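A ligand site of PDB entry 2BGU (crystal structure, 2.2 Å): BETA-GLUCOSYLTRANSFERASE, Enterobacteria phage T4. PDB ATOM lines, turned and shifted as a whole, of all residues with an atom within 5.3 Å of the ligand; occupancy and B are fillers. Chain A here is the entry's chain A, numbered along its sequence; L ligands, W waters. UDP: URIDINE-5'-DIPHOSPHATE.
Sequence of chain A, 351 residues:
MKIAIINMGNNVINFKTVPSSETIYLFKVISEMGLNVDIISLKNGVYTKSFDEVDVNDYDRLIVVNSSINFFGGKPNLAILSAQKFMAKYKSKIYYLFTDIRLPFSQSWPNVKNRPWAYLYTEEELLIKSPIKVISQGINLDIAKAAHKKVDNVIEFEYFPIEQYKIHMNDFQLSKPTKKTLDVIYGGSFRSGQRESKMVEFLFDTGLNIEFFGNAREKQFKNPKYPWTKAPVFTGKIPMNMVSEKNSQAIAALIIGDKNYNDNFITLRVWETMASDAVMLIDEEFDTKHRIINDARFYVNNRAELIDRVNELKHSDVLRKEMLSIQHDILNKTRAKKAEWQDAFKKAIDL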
ATOM      1  N   VAL A  18      -1.685  -3.340   3.360  1.00  0.00           N
ATOM      2  CA  VAL A  18      -2.545  -4.295   4.054  1.00  0.00           C
ATOM      3  C   VAL A  18      -1.966  -5.719   3.993  1.00  0.00           C
ATOM      4  O   VAL A  18      -2.021  -6.458   4.978  1.00  0.00           O
ATOM      5  CB  VAL A  18      -4.023  -4.247   3.536  1.00  0.00           C
ATOM      6  CG1 VAL A  18      -4.821  -5.443   4.031  1.00  0.00           C
ATOM      7  CG2 VAL A  18      -4.691  -2.982   4.038  1.00  0.00           C
ATOM      8  N   ASP A 100      -8.806 -15.898   0.582  1.00  0.00           N
ATOM      9  CA  ASP A 100      -9.586 -15.118  -0.362  1.00  0.00           C
ATOM     10  C   ASP A 100      -9.873 -16.052  -1.518  1.00  0.00           C
ATOM     11  O   ASP A 100      -8.943 -16.670  -2.050  1.00  0.00           O
ATOM     12  CB  ASP A 100      -8.754 -13.907  -0.834  1.00  0.00           C
ATOM     13  CG  ASP A 100      -9.591 -12.823  -1.511  1.00  0.00           C
ATOM     14  OD1 ASP A 100     -10.403 -13.152  -2.391  1.00  0.00           O
ATOM     15  OD2 ASP A 100      -9.391 -11.636  -1.185  1.00  0.00           O
ATOM     16  N   LYS A 166      -7.353 -11.822  14.647  1.00  0.00           N
ATOM     17  CA  LYS A 166      -7.417 -10.460  15.145  1.00  0.00           C
ATOM     18  C   LYS A 166      -7.959 -10.410  16.561  1.00  0.00           C
ATOM     19  O   LYS A 166      -7.381  -9.748  17.423  1.00  0.00           O
ATOM     20  CB  LYS A 166      -8.287  -9.593  14.218  1.00  0.00           C
ATOM     21  CG  LYS A 166      -8.042  -8.081  14.364  1.00  0.00           C
ATOM     22  CD  LYS A 166      -8.679  -7.275  13.218  1.00  0.00           C
ATOM     23  CE  LYS A 166      -8.119  -5.827  13.137  1.00  0.00           C
ATOM     24  NZ  LYS A 166      -8.422  -5.158  11.815  1.00  0.00           N
ATOM     25  N   TYR A 186     -19.059   1.106   5.438  1.00  0.00           N
ATOM     26  CA  TYR A 186     -18.510  -0.111   4.867  1.00  0.00           C
ATOM     27  C   TYR A 186     -17.091   0.181   4.406  1.00  0.00           C
ATOM     28  O   TYR A 186     -16.853   1.165   3.720  1.00  0.00           O
ATOM     29  CB  TYR A 186     -19.367  -0.579   3.685  1.00  0.00           C
ATOM     30  CG  TYR A 186     -18.819  -1.803   2.951  1.00  0.00           C
ATOM     31  CD1 TYR A 186     -19.126  -3.090   3.385  1.00  0.00           C
ATOM     32  CD2 TYR A 186     -18.000  -1.662   1.842  1.00  0.00           C
ATOM     33  CE1 TYR A 186     -18.622  -4.219   2.722  1.00  0.00           C
ATOM     34  CE2 TYR A 186     -17.487  -2.766   1.183  1.00  0.00           C
ATOM     35  CZ  TYR A 186     -17.812  -4.039   1.617  1.00  0.00           C
ATOM     36  OH  TYR A 186     -17.303  -5.131   0.939  1.00  0.00           O
ATOM     37  N   GLY A 187     -16.136  -0.655   4.806  1.00  0.00           N
ATOM     38  CA  GLY A 187     -14.767  -0.425   4.366  1.00  0.00           C
ATOM     39  C   GLY A 187     -14.231  -1.590   3.558  1.00  0.00           C
ATOM     40  O   GLY A 187     -14.384  -2.748   3.943  1.00  0.00           O
ATOM     41  N   GLY A 188     -13.604  -1.288   2.431  1.00  0.00           N
ATOM     42  CA  GLY A 188     -13.049  -2.353   1.616  1.00  0.00           C
ATOM     43  C   GLY A 188     -12.646  -1.870   0.250  1.00  0.00           C
ATOM     44  O   GLY A 188     -12.571  -0.653   0.000  1.00  0.00           O
ATOM     45  N   SER A 189     -12.407  -2.806  -0.652  1.00  0.00           N
ATOM     46  CA  SER A 189     -12.021  -2.447  -2.004  1.00  0.00           C
ATOM     47  C   SER A 189     -13.102  -2.891  -2.990  1.00  0.00           C
ATOM     48  O   SER A 189     -14.100  -3.492  -2.591  1.00  0.00           O
ATOM     49  CB  SER A 189     -10.652  -3.063  -2.336  1.00  0.00           C
ATOM     50  OG  SER A 189     -10.707  -4.469  -2.341  1.00  0.00           O
ATOM     51  N   ARG A 191     -12.906  -5.135  -5.246  1.00  0.00           N
ATOM     52  CA  ARG A 191     -12.848  -6.560  -5.490  1.00  0.00           C
ATOM     53  C   ARG A 191     -13.126  -6.871  -6.941  1.00  0.00           C
ATOM     54  O   ARG A 191     -13.861  -7.805  -7.248  1.00  0.00           O
ATOM     55  CB  ARG A 191     -13.822  -7.313  -4.584  1.00  0.00           C
ATOM     56  CG  ARG A 191     -13.398  -7.287  -3.141  1.00  0.00           C
ATOM     57  CD  ARG A 191     -14.197  -8.257  -2.325  1.00  0.00           C
ATOM     58  NE  ARG A 191     -14.019  -9.633  -2.770  1.00  0.00           N
ATOM     59  CZ  ARG A 191     -12.946 -10.382  -2.527  1.00  0.00           C
ATOM     60  NH1 ARG A 191     -11.911  -9.895  -1.849  1.00  0.00           N
ATOM     61  NH2 ARG A 191     -12.919 -11.652  -2.894  1.00  0.00           N
ATOM     62  N   ARG A 195     -18.471  -7.990  -6.138  1.00  0.00           N
ATOM     63  CA  ARG A 195     -19.686  -7.837  -5.362  1.00  0.00           C
ATOM     64  C   ARG A 195     -20.357  -6.494  -5.647  1.00  0.00           C
ATOM     65  O   ARG A 195     -21.014  -5.927  -4.777  1.00  0.00           O
ATOM     66  CB  ARG A 195     -19.452  -8.074  -3.859  1.00  0.00           C
ATOM     67  CG  ARG A 195     -18.613  -7.070  -3.156  1.00  0.00           C
ATOM     68  CD  ARG A 195     -18.467  -7.417  -1.680  1.00  0.00           C
ATOM     69  NE  ARG A 195     -17.659  -8.615  -1.462  1.00  0.00           N
ATOM     70  CZ  ARG A 195     -16.960  -8.865  -0.365  1.00  0.00           C
ATOM     71  NH1 ARG A 195     -16.935  -8.006   0.639  1.00  0.00           N
ATOM     72  NH2 ARG A 195     -16.264  -9.973  -0.272  1.00  0.00           N
ATOM     73  N   PHE A 213     -15.282   3.553   2.869  1.00  0.00           N
ATOM     74  CA  PHE A 213     -13.867   3.857   2.934  1.00  0.00           C
ATOM     75  C   PHE A 213     -13.063   2.716   2.352  1.00  0.00           C
ATOM     76  O   PHE A 213     -13.577   1.611   2.165  1.00  0.00           O
ATOM     77  CB  PHE A 213     -13.427   4.231   4.360  1.00  0.00           C
ATOM     78  CG  PHE A 213     -13.485   3.094   5.357  1.00  0.00           C
ATOM     79  CD1 PHE A 213     -14.653   2.819   6.031  1.00  0.00           C
ATOM     80  CD2 PHE A 213     -12.339   2.365   5.666  1.00  0.00           C
ATOM     81  CE1 PHE A 213     -14.693   1.849   7.029  1.00  0.00           C
ATOM     82  CE2 PHE A 213     -12.366   1.392   6.654  1.00  0.00           C
ATOM     83  CZ  PHE A 213     -13.547   1.120   7.339  1.00  0.00           C
ATOM     84  N   GLY A 214     -11.823   3.008   1.985  1.00  0.00           N
ATOM     85  CA  GLY A 214     -10.960   1.999   1.402  1.00  0.00           C
ATOM     86  C   GLY A 214     -10.506   2.365   0.003  1.00  0.00           C
ATOM     87  O   GLY A 214     -10.422   3.540  -0.353  1.00  0.00           O
ATOM     88  N   ASN A 215     -10.230   1.358  -0.806  1.00  0.00           N
ATOM     89  CA  ASN A 215      -9.740   1.558  -2.163  1.00  0.00           C
ATOM     90  C   ASN A 215     -10.760   1.757  -3.289  1.00  0.00           C
ATOM     91  O   ASN A 215     -10.365   2.009  -4.422  1.00  0.00           O
ATOM     92  CB  ASN A 215      -8.783   0.407  -2.548  1.00  0.00           C
ATOM     93  N   GLY A 236     -10.665   7.764   1.631  1.00  0.00           N
ATOM     94  CA  GLY A 236      -9.485   6.933   1.456  1.00  0.00           C
ATOM     95  C   GLY A 236      -9.299   5.769   2.399  1.00  0.00           C
ATOM     96  O   GLY A 236     -10.063   5.594   3.354  1.00  0.00           O
ATOM     97  N   LYS A 237      -8.255   4.976   2.152  1.00  0.00           N
ATOM     98  CA  LYS A 237      -7.961   3.822   2.989  1.00  0.00           C
ATOM     99  C   LYS A 237      -7.278   4.234   4.278  1.00  0.00           C
ATOM    100  O   LYS A 237      -6.610   5.262   4.332  1.00  0.00           O
ATOM    101  CB  LYS A 237      -7.119   2.774   2.239  1.00  0.00           C
ATOM    102  CG  LYS A 237      -5.805   3.293   1.691  1.00  0.00           C
ATOM    103  N   ILE A 238      -7.496   3.450   5.322  1.00  0.00           N
ATOM    104  CA  ILE A 238      -6.917   3.659   6.642  1.00  0.00           C
ATOM    105  C   ILE A 238      -6.142   2.381   7.020  1.00  0.00           C
ATOM    106  O   ILE A 238      -6.297   1.353   6.353  1.00  0.00           O
ATOM    107  CB  ILE A 238      -8.023   3.918   7.698  1.00  0.00           C
ATOM    108  CG1 ILE A 238      -8.883   2.666   7.881  1.00  0.00           C
ATOM    109  CG2 ILE A 238      -8.907   5.088   7.272  1.00  0.00           C
ATOM    110  CD1 ILE A 238      -9.747   2.731   9.074  1.00  0.00           C
ATOM    111  N   PRO A 239      -5.258   2.450   8.043  1.00  0.00           N
ATOM    112  CA  PRO A 239      -4.507   1.239   8.428  1.00  0.00           C
ATOM    113  C   PRO A 239      -5.425   0.153   9.003  1.00  0.00           C
ATOM    114  O   PRO A 239      -6.412   0.458   9.666  1.00  0.00           O
ATOM    115  CB  PRO A 239      -3.547   1.770   9.501  1.00  0.00           C
ATOM    116  CG  PRO A 239      -3.318   3.184   9.090  1.00  0.00           C
ATOM    117  CD  PRO A 239      -4.712   3.632   8.736  1.00  0.00           C
ATOM    118  N   MET A 240      -5.042  -1.095   8.784  1.00  0.00           N
ATOM    119  CA  MET A 240      -5.803  -2.228   9.279  1.00  0.00           C
ATOM    120  C   MET A 240      -6.164  -2.054  10.728  1.00  0.00           C
ATOM    121  O   MET A 240      -7.276  -2.361  11.118  1.00  0.00           O
ATOM    122  CB  MET A 240      -4.995  -3.516   9.163  1.00  0.00           C
ATOM    123  CG  MET A 240      -5.112  -4.247   7.878  1.00  0.00           C
ATOM    124  SD  MET A 240      -4.608  -5.967   8.130  1.00  0.00           S
ATOM    125  CE  MET A 240      -5.935  -6.597   9.148  1.00  0.00           C
ATOM    126  N   VAL A 243      -9.494   0.149  11.509  1.00  0.00           N
ATOM    127  CA  VAL A 243     -10.801  -0.258  11.012  1.00  0.00           C
ATOM    128  C   VAL A 243     -11.975  -0.277  12.011  1.00  0.00           C
ATOM    129  O   VAL A 243     -13.004   0.307  11.718  1.00  0.00           O
ATOM    130  CB  VAL A 243     -10.688  -1.562  10.190  1.00  0.00           C
ATOM    131  CG1 VAL A 243     -12.060  -2.057   9.771  1.00  0.00           C
ATOM    132  CG2 VAL A 243      -9.810  -1.312   8.966  1.00  0.00           C
ATOM    133  N   ILE A 256     -21.343  -7.906   3.850  1.00  0.00           N
ATOM    134  CA  ILE A 256     -21.758  -8.521   2.587  1.00  0.00           C
ATOM    135  C   ILE A 256     -20.552  -9.319   2.104  1.00  0.00           C
ATOM    136  O   ILE A 256     -19.475  -9.208   2.686  1.00  0.00           O
ATOM    137  CB  ILE A 256     -22.156  -7.483   1.479  1.00  0.00           C
ATOM    138  CG1 ILE A 256     -21.147  -6.345   1.398  1.00  0.00           C
ATOM    139  CG2 ILE A 256     -23.551  -6.948   1.700  1.00  0.00           C
ATOM    140  CD1 ILE A 256     -21.286  -5.563   0.118  1.00  0.00           C
ATOM    141  N   TYR A 261     -18.774 -16.813  -0.815  1.00  0.00           N
ATOM    142  CA  TYR A 261     -18.516 -16.611   0.602  1.00  0.00           C
ATOM    143  C   TYR A 261     -19.785 -16.923   1.348  1.00  0.00           C
ATOM    144  O   TYR A 261     -19.738 -17.257   2.529  1.00  0.00           O
ATOM    145  CB  TYR A 261     -18.142 -15.161   0.897  1.00  0.00           C
ATOM    146  CG  TYR A 261     -16.708 -14.819   0.584  1.00  0.00           C
ATOM    147  CD1 TYR A 261     -15.876 -15.738  -0.040  1.00  0.00           C
ATOM    148  CD2 TYR A 261     -16.188 -13.582   0.940  1.00  0.00           C
ATOM    149  CE1 TYR A 261     -14.563 -15.427  -0.331  1.00  0.00           C
ATOM    150  CE2 TYR A 261     -14.870 -13.257   0.650  1.00  0.00           C
ATOM    151  CZ  TYR A 261     -14.056 -14.184   0.014  1.00  0.00           C
ATOM    152  OH  TYR A 261     -12.742 -13.872  -0.287  1.00  0.00           O
ATOM    153  N   THR A 267     -15.575 -13.672   7.337  1.00  0.00           N
ATOM    154  CA  THR A 267     -14.447 -12.832   7.012  1.00  0.00           C
ATOM    155  C   THR A 267     -13.990 -11.970   8.176  1.00  0.00           C
ATOM    156  O   THR A 267     -14.708 -11.797   9.166  1.00  0.00           O
ATOM    157  CB  THR A 267     -14.773 -11.959   5.786  1.00  0.00           C
ATOM    158  OG1 THR A 267     -16.063 -11.354   5.959  1.00  0.00           O
ATOM    159  CG2 THR A 267     -14.805 -12.819   4.529  1.00  0.00           C
ATOM    160  N   LEU A 268     -12.784 -11.437   8.049  1.00  0.00           N
ATOM    161  CA  LEU A 268     -12.223 -10.576   9.086  1.00  0.00           C
ATOM    162  C   LEU A 268     -13.177  -9.394   9.394  1.00  0.00           C
ATOM    163  O   LEU A 268     -13.303  -9.001  10.547  1.00  0.00           O
ATOM    164  CB  LEU A 268     -10.837 -10.088   8.638  1.00  0.00           C
ATOM    165  CG  LEU A 268      -9.924  -9.358   9.633  1.00  0.00           C
ATOM    166  CD1 LEU A 268      -9.638 -10.215  10.839  1.00  0.00           C
ATOM    167  CD2 LEU A 268      -8.662  -8.975   8.935  1.00  0.00           C
ATOM    168  N   ARG A 269     -13.885  -8.876   8.381  1.00  0.00           N
ATOM    169  CA  ARG A 269     -14.814  -7.775   8.620  1.00  0.00           C
ATOM    170  C   ARG A 269     -15.890  -8.109   9.664  1.00  0.00           C
ATOM    171  O   ARG A 269     -16.329  -7.214  10.412  1.00  0.00           O
ATOM    172  CB  ARG A 269     -15.426  -7.235   7.330  1.00  0.00           C
ATOM    173  CG  ARG A 269     -16.562  -7.988   6.757  1.00  0.00           C
ATOM    174  CD  ARG A 269     -17.308  -7.127   5.734  1.00  0.00           C
ATOM    175  NE  ARG A 269     -16.470  -6.792   4.589  1.00  0.00           N
ATOM    176  CZ  ARG A 269     -15.926  -5.598   4.376  1.00  0.00           C
ATOM    177  NH1 ARG A 269     -16.158  -4.594   5.206  1.00  0.00           N
ATOM    178  NH2 ARG A 269     -15.158  -5.388   3.324  1.00  0.00           N
ATOM    179  N   GLU A 272     -14.094  -7.309  12.882  1.00  0.00           N
ATOM    180  CA  GLU A 272     -13.775  -5.889  12.979  1.00  0.00           C
ATOM    181  C   GLU A 272     -15.058  -5.124  13.273  1.00  0.00           C
ATOM    182  O   GLU A 272     -15.039  -4.126  13.992  1.00  0.00           O
ATOM    183  CB  GLU A 272     -13.200  -5.380  11.674  1.00  0.00           C
ATOM    184  CG  GLU A 272     -11.820  -5.894  11.384  1.00  0.00           C
ATOM    185  CD  GLU A 272     -11.396  -5.576   9.979  1.00  0.00           C
ATOM    186  OE1 GLU A 272     -12.283  -5.425   9.114  1.00  0.00           O
ATOM    187  OE2 GLU A 272     -10.182  -5.480   9.737  1.00  0.00           O
HETATM  188  N1  UDP L   1      -9.205  -2.707   5.118  1.00  0.00           N
HETATM  189  C2  UDP L   1      -8.236  -1.875   5.613  1.00  0.00           C
HETATM  190  N3  UDP L   1      -8.330  -0.539   5.330  1.00  0.00           N
HETATM  191  C4  UDP L   1      -9.327   0.007   4.581  1.00  0.00           C
HETATM  192  C5  UDP L   1     -10.508  -0.791   4.121  1.00  0.00           C
HETATM  193  C6  UDP L   1     -10.375  -2.124   4.345  1.00  0.00           C
HETATM  194  O2  UDP L   1      -7.323  -2.289   6.315  1.00  0.00           O
HETATM  195  O4  UDP L   1      -9.273   1.179   4.213  1.00  0.00           O
HETATM  196  C1' UDP L   1      -9.078  -4.173   5.285  1.00  0.00           C
HETATM  197  C2' UDP L   1      -9.925  -4.556   6.423  1.00  0.00           C
HETATM  198  O2' UDP L   1      -9.267  -5.461   7.317  1.00  0.00           O
HETATM  199  C3' UDP L   1     -11.184  -5.071   5.774  1.00  0.00           C
HETATM  200  C4' UDP L   1     -10.658  -5.719   4.606  1.00  0.00           C
HETATM  201  O4' UDP L   1      -9.695  -4.769   4.148  1.00  0.00           O
HETATM  202  O3' UDP L   1     -11.893  -5.994   6.589  1.00  0.00           O
HETATM  203  C5' UDP L   1     -11.720  -5.904   3.602  1.00  0.00           C
HETATM  204  O5' UDP L   1     -11.125  -6.455   2.379  1.00  0.00           O
HETATM  205  PA  UDP L   1     -12.055  -6.690   1.092  1.00  0.00           P
HETATM  206  O1A UDP L   1     -12.434  -5.408   0.569  1.00  0.00           O
HETATM  207  O2A UDP L   1     -11.183  -7.349   0.118  1.00  0.00           O
HETATM  208  O3A UDP L   1     -13.330  -7.571   1.405  1.00  0.00           O
HETATM  209  PB  UDP L   1     -13.786  -8.860   2.215  1.00  0.00           P
HETATM  210  O1B UDP L   1     -12.939  -9.086   3.281  1.00  0.00           O
HETATM  211  O2B UDP L   1     -13.683  -9.986   1.264  1.00  0.00           O
HETATM  212  O3B UDP L   1     -15.108  -8.602   2.859  1.00  0.00           O
HETATM  213  O   HOH W   1      -7.720  -7.686   5.169  1.00  0.00           O
HETATM  214  O   HOH W   2     -17.207 -10.119   3.917  1.00  0.00           O
HETATM  215  O   HOH W   3      -9.050  -7.056  -1.604  1.00  0.00           O
HETATM  216  O   HOH W   4     -12.915  -8.823   5.795  1.00  0.00           O
HETATM  217  O   HOH W   5     -14.932  -4.950  -0.364  1.00  0.00           O
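Water W4 lies within hydrogen-bond range of an oxygen (O1B) of the ligand (2.5 Å), the backbone NH of Arg 269 (2.8 Å) and the backbone NH of Leu 268 (3.5 Å). Water W5 lies within hydrogen-bond range of an oxygen (O1A) of the ligand (2.7 Å), the side-chain hydroxyl (OH) of Tyr 186 (2.7 Å) and the backbone carbonyl oxygen (O) of Ser 189 (2.8 Å). Water W3 bridges an oxygen (O2A) of the ligand (2.8 Å) and the side-chain hydroxyl of Ser 189 (3.2 Å). Water W2 lies within hydrogen-bond range of the side-chain hydroxyl of Thr 267, the backbone carbonyl oxygen of Ile 256, an oxygen (O3B) of the ligand and the guanidinium group of Arg 269.
O of Gly 188 is in hydrogen-bond range of N of Asn 215. The side-chain carboxylate (OD1) of Asp 100 sits at hydrogen-bond distance from the side-chain hydroxyl (OH) of Tyr 261 (3.2 Å). The side-chain carboxylate of Glu 272 is in salt-bridge range of the side-chain amino group of Lys 166, 2.7 Å away. NH2 of Arg 191 sits at hydrogen-bond distance from OH of Tyr 261, at 3.4 Å. N of Gly 214 sits at hydrogen-bond distance from O of Gly 236 (3.4 Å). OD1 of Asp 100 lies within salt-bridge range of NH2 of Arg 191 (3.0 Å). O of Phe 213 lies within hydrogen-bond range of N of Gly 188 (2.9 Å). The guanidinium group of Arg 269 is in hydrogen-bond range of the side-chain hydroxyl of Tyr 186 (3.2 Å).
CG2 of Val 18 touches O2 of the ligand, at 3.5 Å. Gly 187 touches the ligand (C to C5, 3.8 Å). CA of Gly 188 touches O1A of the ligand, at 3.3 Å. Phe 213 touches the ligand (CD2 to O4, 3.6 Å). Gly 214 touches the ligand. Lys 237 touches the ligand. Met 240 touches the ligand. CG2 of Val 243 touches C2 of the ligand, 3.7 Å away. CE2 of Tyr 261 touches O2B of the ligand (3.5 Å). CD2 of Leu 268 touches O2' of the ligand, at 3.9 Å. 16 residues have an atom within 4 Å of the ligand: Val 18, Gly 187, Gly 188, Ser 189, Arg 191, Arg 195, Phe 213, Gly 214, Lys 237, Ile 238, Met 240, Val 243, Tyr 261, Leu 268, Arg 269 and Glu 272.
The guanidinium group (NE) of Arg 269 is in salt-bridge range of an oxygen (O3B) of the ligand (2.9 Å). O of Ile 238 sits at hydrogen-bond distance from N3 of the ligand (3.0 Å). NH1 of Arg 191 is in salt-bridge range of O2A of the ligand (3.3 Å). An oxygen (O3B) of the ligand lies within salt-bridge range of the guanidinium group (NH1) of Arg 195 (2.9 Å). The side-chain carboxylate (OE2) of Glu 272 lies within hydrogen-bond range of an oxygen (O2') of the ligand (2.6 Å). N of Ser 189 lies within hydrogen-bond range of O1A of the ligand (2.9 Å). The backbone NH (N) of Ile 238 sits at hydrogen-bond distance from an oxygen (O4) of the ligand.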
